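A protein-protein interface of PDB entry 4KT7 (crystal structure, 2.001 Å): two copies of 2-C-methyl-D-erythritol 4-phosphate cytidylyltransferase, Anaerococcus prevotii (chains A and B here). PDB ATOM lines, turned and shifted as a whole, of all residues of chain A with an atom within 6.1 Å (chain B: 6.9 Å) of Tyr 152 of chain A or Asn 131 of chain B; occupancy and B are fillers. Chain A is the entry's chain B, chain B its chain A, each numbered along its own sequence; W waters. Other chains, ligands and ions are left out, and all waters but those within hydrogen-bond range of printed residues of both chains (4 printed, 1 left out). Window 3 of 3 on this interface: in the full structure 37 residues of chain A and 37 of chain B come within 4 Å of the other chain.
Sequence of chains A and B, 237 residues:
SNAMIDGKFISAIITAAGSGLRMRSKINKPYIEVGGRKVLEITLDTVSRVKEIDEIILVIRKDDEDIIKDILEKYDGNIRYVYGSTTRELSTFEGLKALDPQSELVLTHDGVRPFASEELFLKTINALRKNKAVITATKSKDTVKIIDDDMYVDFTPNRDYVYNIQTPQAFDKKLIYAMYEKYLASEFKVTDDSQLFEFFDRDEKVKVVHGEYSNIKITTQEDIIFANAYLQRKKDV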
ATOM      1  N   ILE A 146       0.915   5.410   0.165  1.00  0.00           N
ATOM      2  CA  ILE A 146       1.798   5.397   1.330  1.00  0.00           C
ATOM      3  C   ILE A 146       0.934   5.887   2.476  1.00  0.00           C
ATOM      4  O   ILE A 146       0.248   6.906   2.372  1.00  0.00           O
ATOM      5  CB  ILE A 146       2.998   6.332   1.174  1.00  0.00           C
ATOM      6  CG1 ILE A 146       3.766   5.988  -0.095  1.00  0.00           C
ATOM      7  CG2 ILE A 146       3.947   6.256   2.421  1.00  0.00           C
ATOM      8  CD1 ILE A 146       4.275   4.557  -0.120  1.00  0.00           C
ATOM      9  N   ILE A 147       0.918   5.137   3.569  1.00  0.00           N
ATOM     10  CA  ILE A 147       0.052   5.493   4.677  1.00  0.00           C
ATOM     11  C   ILE A 147       0.919   5.775   5.889  1.00  0.00           C
ATOM     12  O   ILE A 147       2.074   5.347   5.931  1.00  0.00           O
ATOM     13  CB  ILE A 147      -0.927   4.367   4.969  1.00  0.00           C
ATOM     14  CG1 ILE A 147      -0.183   3.165   5.528  1.00  0.00           C
ATOM     15  CG2 ILE A 147      -1.694   3.978   3.689  1.00  0.00           C
ATOM     16  CD1 ILE A 147      -0.983   2.425   6.553  1.00  0.00           C
ATOM     17  N   ASP A 148       0.385   6.522   6.854  1.00  0.00           N
ATOM     18  CA  ASP A 148       1.148   6.896   8.051  1.00  0.00           C
ATOM     19  C   ASP A 148       0.917   5.934   9.213  1.00  0.00           C
ATOM     20  O   ASP A 148       0.177   4.957   9.085  1.00  0.00           O
ATOM     21  CB  ASP A 148       0.931   8.369   8.464  1.00  0.00           C
ATOM     22  CG  ASP A 148      -0.458   8.647   9.009  1.00  0.00           C
ATOM     23  OD1 ASP A 148      -1.190   7.695   9.386  1.00  0.00           O
ATOM     24  OD2 ASP A 148      -0.816   9.846   9.088  1.00  0.00           O
ATOM     25  N   ASP A 149       1.552   6.207  10.348  1.00  0.00           N
ATOM     26  CA  ASP A 149       1.499   5.273  11.469  1.00  0.00           C
ATOM     27  C   ASP A 149       0.173   5.330  12.229  1.00  0.00           C
ATOM     28  O   ASP A 149      -0.015   4.586  13.187  1.00  0.00           O
ATOM     29  CB  ASP A 149       2.697   5.480  12.415  1.00  0.00           C
ATOM     30  CG  ASP A 149       2.788   6.902  12.949  1.00  0.00           C
ATOM     31  OD1 ASP A 149       2.141   7.806  12.370  1.00  0.00           O
ATOM     32  OD2 ASP A 149       3.514   7.118  13.946  1.00  0.00           O
ATOM     33  N   ASP A 150      -0.743   6.200  11.800  1.00  0.00           N
ATOM     34  CA  ASP A 150      -2.084   6.254  12.390  1.00  0.00           C
ATOM     35  C   ASP A 150      -3.161   5.741  11.412  1.00  0.00           C
ATOM     36  O   ASP A 150      -4.368   6.000  11.597  1.00  0.00           O
ATOM     37  CB  ASP A 150      -2.414   7.672  12.855  1.00  0.00           C
ATOM     38  CG  ASP A 150      -1.584   8.101  14.063  1.00  0.00           C
ATOM     39  OD1 ASP A 150      -1.302   7.252  14.933  1.00  0.00           O
ATOM     40  OD2 ASP A 150      -1.213   9.288  14.150  1.00  0.00           O
ATOM     41  N   MET A 151      -2.712   5.014  10.391  1.00  0.00           N
ATOM     42  CA  MET A 151      -3.587   4.427   9.369  1.00  0.00           C
ATOM     43  C   MET A 151      -4.419   5.522   8.698  1.00  0.00           C
ATOM     44  O   MET A 151      -5.633   5.386   8.548  1.00  0.00           O
ATOM     45  CB  MET A 151      -4.505   3.348   9.979  1.00  0.00           C
ATOM     46  CG  MET A 151      -3.765   2.120  10.494  1.00  0.00           C
ATOM     47  SD  MET A 151      -3.048   1.134   8.978  1.00  0.00           S
ATOM     48  CE  MET A 151      -4.737   0.406   8.324  1.00  0.00           C
ATOM     49  N   TYR A 152      -3.759   6.625   8.347  1.00  0.00           N
ATOM     50  CA  TYR A 152      -4.327   7.627   7.449  1.00  0.00           C
ATOM     51  C   TYR A 152      -3.440   7.691   6.220  1.00  0.00           C
ATOM     52  O   TYR A 152      -2.231   7.448   6.313  1.00  0.00           O
ATOM     53  CB  TYR A 152      -4.365   9.006   8.121  1.00  0.00           C
ATOM     54  CG  TYR A 152      -5.407   9.120   9.200  1.00  0.00           C
ATOM     55  CD1 TYR A 152      -6.711   9.447   8.887  1.00  0.00           C
ATOM     56  CD2 TYR A 152      -5.090   8.898  10.524  1.00  0.00           C
ATOM     57  CE1 TYR A 152      -7.673   9.558   9.861  1.00  0.00           C
ATOM     58  CE2 TYR A 152      -6.051   8.993  11.514  1.00  0.00           C
ATOM     59  CZ  TYR A 152      -7.342   9.323  11.175  1.00  0.00           C
ATOM     60  OH  TYR A 152      -8.308   9.426  12.152  1.00  0.00           O
ATOM     61  N   VAL A 153      -4.021   8.004   5.065  1.00  0.00           N
ATOM     62  CA  VAL A 153      -3.211   8.131   3.860  1.00  0.00           C
ATOM     63  C   VAL A 153      -2.206   9.271   4.015  1.00  0.00           C
ATOM     64  O   VAL A 153      -2.573  10.368   4.467  1.00  0.00           O
ATOM     65  CB  VAL A 153      -4.090   8.359   2.609  1.00  0.00           C
ATOM     66  CG1 VAL A 153      -3.221   8.744   1.366  1.00  0.00           C
ATOM     67  CG2 VAL A 153      -4.939   7.112   2.341  1.00  0.00           C
ATOM     68  N   ASP A 154      -0.933   9.008   3.680  1.00  0.00           N
ATOM     69  CA  ASP A 154       0.074  10.073   3.594  1.00  0.00           C
ATOM     70  C   ASP A 154      -0.057  10.706   2.215  1.00  0.00           C
ATOM     71  O   ASP A 154      -0.374  11.888   2.082  1.00  0.00           O
ATOM     72  CB  ASP A 154       1.492   9.516   3.776  1.00  0.00           C
ATOM     73  CG  ASP A 154       2.169  10.023   5.033  1.00  0.00           C
ATOM     74  OD1 ASP A 154       1.709  11.036   5.616  1.00  0.00           O
ATOM     75  OD2 ASP A 154       3.169   9.398   5.452  1.00  0.00           O
ATOM     76  N   LEU B 105     -24.356   9.956   3.846  1.00  0.00           N
ATOM     77  CA  LEU B 105     -23.117   9.168   3.768  1.00  0.00           C
ATOM     78  C   LEU B 105     -23.185   8.238   2.568  1.00  0.00           C
ATOM     79  O   LEU B 105     -24.245   7.689   2.283  1.00  0.00           O
ATOM     80  CB  LEU B 105     -22.935   8.339   5.045  1.00  0.00           C
ATOM     81  CG  LEU B 105     -22.827   9.102   6.363  1.00  0.00           C
ATOM     82  CD1 LEU B 105     -22.979   8.163   7.563  1.00  0.00           C
ATOM     83  CD2 LEU B 105     -21.512   9.875   6.445  1.00  0.00           C
ATOM     84  N   ASN B 126     -18.376   2.014   9.965  1.00  0.00           N
ATOM     85  CA  ASN B 126     -18.049   2.491  11.312  1.00  0.00           C
ATOM     86  C   ASN B 126     -16.894   3.496  11.359  1.00  0.00           C
ATOM     87  O   ASN B 126     -16.815   4.297  12.285  1.00  0.00           O
ATOM     88  CB  ASN B 126     -17.803   1.329  12.273  1.00  0.00           C
ATOM     89  CG  ASN B 126     -19.087   0.590  12.621  1.00  0.00           C
ATOM     90  OD1 ASN B 126     -20.194   1.121  12.444  1.00  0.00           O
ATOM     91  ND2 ASN B 126     -18.951  -0.635  13.119  1.00  0.00           N
ATOM     92  N   ALA B 127     -16.006   3.473  10.368  1.00  0.00           N
ATOM     93  CA  ALA B 127     -14.936   4.457  10.336  1.00  0.00           C
ATOM     94  C   ALA B 127     -15.484   5.861   9.997  1.00  0.00           C
ATOM     95  O   ALA B 127     -14.826   6.875  10.262  1.00  0.00           O
ATOM     96  CB  ALA B 127     -13.858   4.044   9.354  1.00  0.00           C
ATOM     97  N   LEU B 128     -16.691   5.920   9.430  1.00  0.00           N
ATOM     98  CA  LEU B 128     -17.319   7.209   9.126  1.00  0.00           C
ATOM     99  C   LEU B 128     -17.770   7.943  10.375  1.00  0.00           C
ATOM    100  O   LEU B 128     -18.129   9.119  10.304  1.00  0.00           O
ATOM    101  CB  LEU B 128     -18.510   7.040   8.192  1.00  0.00           C
ATOM    102  CG  LEU B 128     -18.189   6.631   6.759  1.00  0.00           C
ATOM    103  CD1 LEU B 128     -19.470   6.096   6.133  1.00  0.00           C
ATOM    104  CD2 LEU B 128     -17.672   7.824   5.989  1.00  0.00           C
ATOM    105  N   ARG B 129     -17.748   7.274  11.526  1.00  0.00           N
ATOM    106  CA  ARG B 129     -18.149   7.936  12.764  1.00  0.00           C
ATOM    107  C   ARG B 129     -17.271   9.151  13.075  1.00  0.00           C
ATOM    108  O   ARG B 129     -17.759  10.175  13.565  1.00  0.00           O
ATOM    109  CB  ARG B 129     -18.146   6.953  13.946  1.00  0.00           C
ATOM    110  CG  ARG B 129     -18.754   7.545  15.226  1.00  0.00           C
ATOM    111  CD  ARG B 129     -18.807   6.525  16.375  1.00  0.00           C
ATOM    112  NE  ARG B 129     -17.494   5.919  16.605  1.00  0.00           N
ATOM    113  CZ  ARG B 129     -16.587   6.400  17.448  1.00  0.00           C
ATOM    114  NH1 ARG B 129     -16.851   7.497  18.150  1.00  0.00           N
ATOM    115  NH2 ARG B 129     -15.421   5.780  17.593  1.00  0.00           N
ATOM    116  N   LYS B 130     -15.979   9.054  12.768  1.00  0.00           N
ATOM    117  CA  LYS B 130     -15.057  10.139  13.089  1.00  0.00           C
ATOM    118  C   LYS B 130     -14.243  10.638  11.900  1.00  0.00           C
ATOM    119  O   LYS B 130     -13.400  11.513  12.053  1.00  0.00           O
ATOM    120  CB  LYS B 130     -14.105   9.700  14.203  1.00  0.00           C
ATOM    121  CG  LYS B 130     -14.788   9.521  15.559  1.00  0.00           C
ATOM    122  CD  LYS B 130     -14.004   8.564  16.443  1.00  0.00           C
ATOM    123  CE  LYS B 130     -12.692   9.165  16.907  1.00  0.00           C
ATOM    124  NZ  LYS B 130     -11.860   8.145  17.616  1.00  0.00           N
ATOM    125  N   ASN B 131     -14.477  10.086  10.717  1.00  0.00           N
ATOM    126  CA  ASN B 131     -13.730  10.514   9.541  1.00  0.00           C
ATOM    127  C   ASN B 131     -14.693  10.805   8.413  1.00  0.00           C
ATOM    128  O   ASN B 131     -15.759  10.186   8.335  1.00  0.00           O
ATOM    129  CB  ASN B 131     -12.786   9.403   9.098  1.00  0.00           C
ATOM    130  CG  ASN B 131     -11.869   8.942  10.214  1.00  0.00           C
ATOM    131  OD1 ASN B 131     -10.887   9.614  10.541  1.00  0.00           O
ATOM    132  ND2 ASN B 131     -12.177   7.773  10.793  1.00  0.00           N
ATOM    133  N   LYS B 132     -14.318  11.708   7.514  1.00  0.00           N
ATOM    134  CA  LYS B 132     -15.202  12.024   6.397  1.00  0.00           C
ATOM    135  C   LYS B 132     -14.845  11.271   5.129  1.00  0.00           C
ATOM    136  O   LYS B 132     -15.583  11.326   4.153  1.00  0.00           O
ATOM    137  CB  LYS B 132     -15.281  13.541   6.179  1.00  0.00           C
ATOM    138  CG  LYS B 132     -15.852  14.265   7.404  1.00  0.00           C
ATOM    139  CD  LYS B 132     -16.407  15.645   7.056  1.00  0.00           C
ATOM    140  CE  LYS B 132     -17.373  16.103   8.146  1.00  0.00           C
ATOM    141  NZ  LYS B 132     -18.216  17.273   7.734  1.00  0.00           N
ATOM    142  N   ALA B 133     -13.718  10.557   5.156  1.00  0.00           N
ATOM    143  CA  ALA B 133     -13.324   9.722   4.029  1.00  0.00           C
ATOM    144  C   ALA B 133     -12.639   8.487   4.576  1.00  0.00           C
ATOM    145  O   ALA B 133     -11.846   8.582   5.514  1.00  0.00           O
ATOM    146  CB  ALA B 133     -12.388  10.479   3.105  1.00  0.00           C
ATOM    147  N   VAL B 134     -12.971   7.329   4.002  1.00  0.00           N
ATOM    148  CA  VAL B 134     -12.495   6.044   4.490  1.00  0.00           C
ATOM    149  C   VAL B 134     -12.194   5.177   3.267  1.00  0.00           C
ATOM    150  O   VAL B 134     -13.001   5.119   2.348  1.00  0.00           O
ATOM    151  CB  VAL B 134     -13.600   5.349   5.312  1.00  0.00           C
ATOM    152  CG1 VAL B 134     -13.104   4.014   5.887  1.00  0.00           C
ATOM    153  CG2 VAL B 134     -14.115   6.273   6.448  1.00  0.00           C
ATOM    154  N   ALA B 170     -15.705   4.932   1.513  1.00  0.00           N
ATOM    155  CA  ALA B 170     -16.925   5.662   1.874  1.00  0.00           C
ATOM    156  C   ALA B 170     -16.615   7.091   2.317  1.00  0.00           C
ATOM    157  O   ALA B 170     -15.504   7.371   2.776  1.00  0.00           O
ATOM    158  CB  ALA B 170     -17.696   4.903   2.976  1.00  0.00           C
ATOM    159  N   PHE B 171     -17.598   7.987   2.183  1.00  0.00           N
ATOM    160  CA  PHE B 171     -17.383   9.431   2.380  1.00  0.00           C
ATOM    161  C   PHE B 171     -18.625  10.111   2.907  1.00  0.00           C
ATOM    162  O   PHE B 171     -19.738   9.600   2.733  1.00  0.00           O
ATOM    163  CB  PHE B 171     -17.036  10.117   1.042  1.00  0.00           C
ATOM    164  CG  PHE B 171     -15.993   9.407   0.268  1.00  0.00           C
ATOM    165  CD1 PHE B 171     -14.648   9.680   0.475  1.00  0.00           C
ATOM    166  CD2 PHE B 171     -16.345   8.425  -0.637  1.00  0.00           C
ATOM    167  CE1 PHE B 171     -13.678   8.980  -0.223  1.00  0.00           C
ATOM    168  CE2 PHE B 171     -15.370   7.734  -1.348  1.00  0.00           C
ATOM    169  CZ  PHE B 171     -14.044   8.009  -1.125  1.00  0.00           C
ATOM    170  N   ASP B 172     -18.415  11.272   3.527  1.00  0.00           N
ATOM    171  CA  ASP B 172     -19.453  12.288   3.730  1.00  0.00           C
ATOM    172  C   ASP B 172     -20.024  12.605   2.350  1.00  0.00           C
ATOM    173  O   ASP B 172     -19.270  12.881   1.407  1.00  0.00           O
ATOM    174  CB  ASP B 172     -18.819  13.536   4.379  1.00  0.00           C
ATOM    175  CG  ASP B 172     -19.827  14.648   4.656  1.00  0.00           C
ATOM    176  OD1 ASP B 172     -20.133  15.417   3.727  1.00  0.00           O
ATOM    177  OD2 ASP B 172     -20.295  14.786   5.803  1.00  0.00           O
ATOM    178  N   GLU B 204      -8.976  17.270   5.504  1.00  0.00           N
ATOM    179  CA  GLU B 204      -9.711  16.129   6.016  1.00  0.00           C
ATOM    180  C   GLU B 204      -8.933  14.880   5.625  1.00  0.00           C
ATOM    181  O   GLU B 204      -8.697  14.616   4.440  1.00  0.00           O
ATOM    182  CB  GLU B 204     -11.130  16.061   5.431  1.00  0.00           C
ATOM    183  CG  GLU B 204     -12.020  17.242   5.802  1.00  0.00           C
ATOM    184  CD  GLU B 204     -12.124  18.267   4.682  1.00  0.00           C
ATOM    185  OE1 GLU B 204     -11.251  18.267   3.777  1.00  0.00           O
ATOM    186  OE2 GLU B 204     -13.089  19.068   4.694  1.00  0.00           O
ATOM    187  N   LYS B 205      -8.535  14.104   6.620  1.00  0.00           N
ATOM    188  CA  LYS B 205      -7.703  12.924   6.366  1.00  0.00           C
ATOM    189  C   LYS B 205      -8.500  11.696   5.921  1.00  0.00           C
ATOM    190  O   LYS B 205      -9.672  11.526   6.289  1.00  0.00           O
ATOM    191  CB  LYS B 205      -6.844  12.608   7.601  1.00  0.00           C
ATOM    192  CG  LYS B 205      -5.806  13.681   7.910  1.00  0.00           C
ATOM    193  CD  LYS B 205      -4.513  13.074   8.470  1.00  0.00           C
ATOM    194  CE  LYS B 205      -3.340  14.033   8.259  1.00  0.00           C
ATOM    195  NZ  LYS B 205      -2.132  13.721   9.078  1.00  0.00           N
ATOM    196  N   VAL B 206      -7.863  10.851   5.108  1.00  0.00           N
ATOM    197  CA  VAL B 206      -8.510   9.668   4.581  1.00  0.00           C
ATOM    198  C   VAL B 206      -8.124   8.507   5.482  1.00  0.00           C
ATOM    199  O   VAL B 206      -6.951   8.154   5.577  1.00  0.00           O
ATOM    200  CB  VAL B 206      -8.082   9.380   3.114  1.00  0.00           C
ATOM    201  CG1 VAL B 206      -8.832   8.144   2.557  1.00  0.00           C
ATOM    202  CG2 VAL B 206      -8.329  10.597   2.243  1.00  0.00           C
ATOM    203  N   LYS B 207      -9.109   7.927   6.165  1.00  0.00           N
ATOM    204  CA  LYS B 207      -8.850   6.843   7.095  1.00  0.00           C
ATOM    205  C   LYS B 207      -8.696   5.540   6.336  1.00  0.00           C
ATOM    206  O   LYS B 207      -9.452   5.250   5.392  1.00  0.00           O
ATOM    207  CB  LYS B 207      -9.993   6.714   8.112  1.00  0.00           C
ATOM    208  CG  LYS B 207      -9.789   5.621   9.158  1.00  0.00           C
ATOM    209  CD  LYS B 207      -8.691   6.038  10.158  1.00  0.00           C
ATOM    210  CE  LYS B 207      -8.222   4.854  10.994  1.00  0.00           C
ATOM    211  NZ  LYS B 207      -7.225   5.310  12.013  1.00  0.00           N
ATOM    212  N   VAL B 208      -7.734   4.725   6.745  1.00  0.00           N
ATOM    213  CA  VAL B 208      -7.531   3.462   6.066  1.00  0.00           C
ATOM    214  C   VAL B 208      -8.055   2.345   6.943  1.00  0.00           C
ATOM    215  O   VAL B 208      -7.750   2.286   8.131  1.00  0.00           O
ATOM    216  CB  VAL B 208      -6.044   3.233   5.758  1.00  0.00           C
ATOM    217  CG1 VAL B 208      -5.855   1.899   5.067  1.00  0.00           C
ATOM    218  CG2 VAL B 208      -5.500   4.370   4.885  1.00  0.00           C
HETATM  219  O   HOH W   1      -5.109  11.617   4.586  1.00  0.00           O
HETATM  220  O   HOH W   2      -1.934  11.257  10.789  1.00  0.00           O
HETATM  221  O   HOH W   3       0.842  12.295   8.676  1.00  0.00           O
HETATM  222  O   HOH W   4      -8.290   6.779  13.999  1.00  0.00           O
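O of Val 206 of chain B sits at hydrogen-bond distance from N of Val 153 of chain A, at 3.0 Å.
OD1 of Asn 131 of chain B is in hydrogen-bond range of OH of Tyr 152 of chain A (3.0 Å).
NZ of Lys 207 of chain B is in hydrogen-bond range of O of Asp 150 of chain A, 3.0 Å away.
O of Met 151 of chain A sits at hydrogen-bond distance from N of Val 208 of chain B (2.8 Å).
The side-chain carboxylate (OD1) of Asp 148 of chain A lies within hydrogen-bond range of the backbone NH (N) of Met 151 of chain A (3.2 Å).
The side-chain carboxylate of Asp 148 of chain A is in hydrogen-bond range of the backbone NH of Tyr 152 of chain A (3.0 Å).
The backbone NH (N) of Lys 207 of chain B is in hydrogen-bond range of the backbone carbonyl oxygen (O) of Ala 133 of chain B (2.9 Å).
The backbone NH of Asp 150 of chain A sits at hydrogen-bond distance from the side-chain carboxylate of Asp 148 of chain A (2.9 Å).
The backbone carbonyl oxygen of Ala 127 of chain B is in hydrogen-bond range of the side-chain amide nitrogen of Asn 131 of chain B.
Among the printed residues, pairs that only touch across the chains: Met 151 of chain A with Lys 207 of chain B (3.5 Å), Tyr 152 of chain A with Lys 205 of chain B (3.4 Å), Tyr 152 of chain A with Val 206 of chain B (3.3 Å), Tyr 152 of chain A with Lys 207 of chain B (3.7 Å) and Val 153 of chain A with Val 208 of chain B (3.8 Å).
Of the printed residues of chain B, Asp 150 of chain A touches Lys 207.
Tyr 152 of chain A touches just these residues of chain B: Asn 131, Lys 205, Val 206 and Lys 207.
Of the printed residues of chain A, Asn 131 of chain B touches Tyr 152 (3.0 Å).
Of the printed residues of chain A, Val 206 of chain B touches Tyr 152 and Val 153.
Of the printed residues of chain A, Lys 207 of chain B touches Asp 150 (3.0 Å), Met 151 (3.5 Å) and Tyr 152 (3.7 Å).
Printed residues of chain A within 4 Å of Val 208 of chain B: Met 151 and Val 153.
The nearest residue of chain B that does not touch Tyr 152 of chain A is Val 208 of chain B (4.1 Å).
Of the 18 printed residues of chain B, 5 touch a printed residue of chain A.
Along chain B the printed residues that touch a printed residue of chain A span positions 131 to 208.
Of the 9 printed residues of chain A, 4 touch a printed residue of chain B.
Hydrophobic or aromatic side chains of chain A that line the printed part of chain B: Met 151, Tyr 152 and Val 153.
No position is printed for both chains.
Of the 9 pairs that touch across the chains among the printed residues, none has its exchanged pair printed and touching as well.
Water W2 bridges the side-chain carboxylate of Asp 148 of chain A (2.5 Å) and the side-chain amino group of Lys 205 of chain B (3.0 Å).
Water W4 lies within hydrogen-bond range of NZ of Lys 207 of chain B (2.7 Å) and OH of Tyr 152 of chain A (3.2 Å).
Water W1 bridges O of Val 153 of chain A and N of Val 206 of chain B.
Water W3 lies within hydrogen-bond range of the side-chain carboxylate of Asp 148 of chain A, the side-chain amino group of Lys 205 of chain B and the side-chain carboxylate of Asp 154 of chain A.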
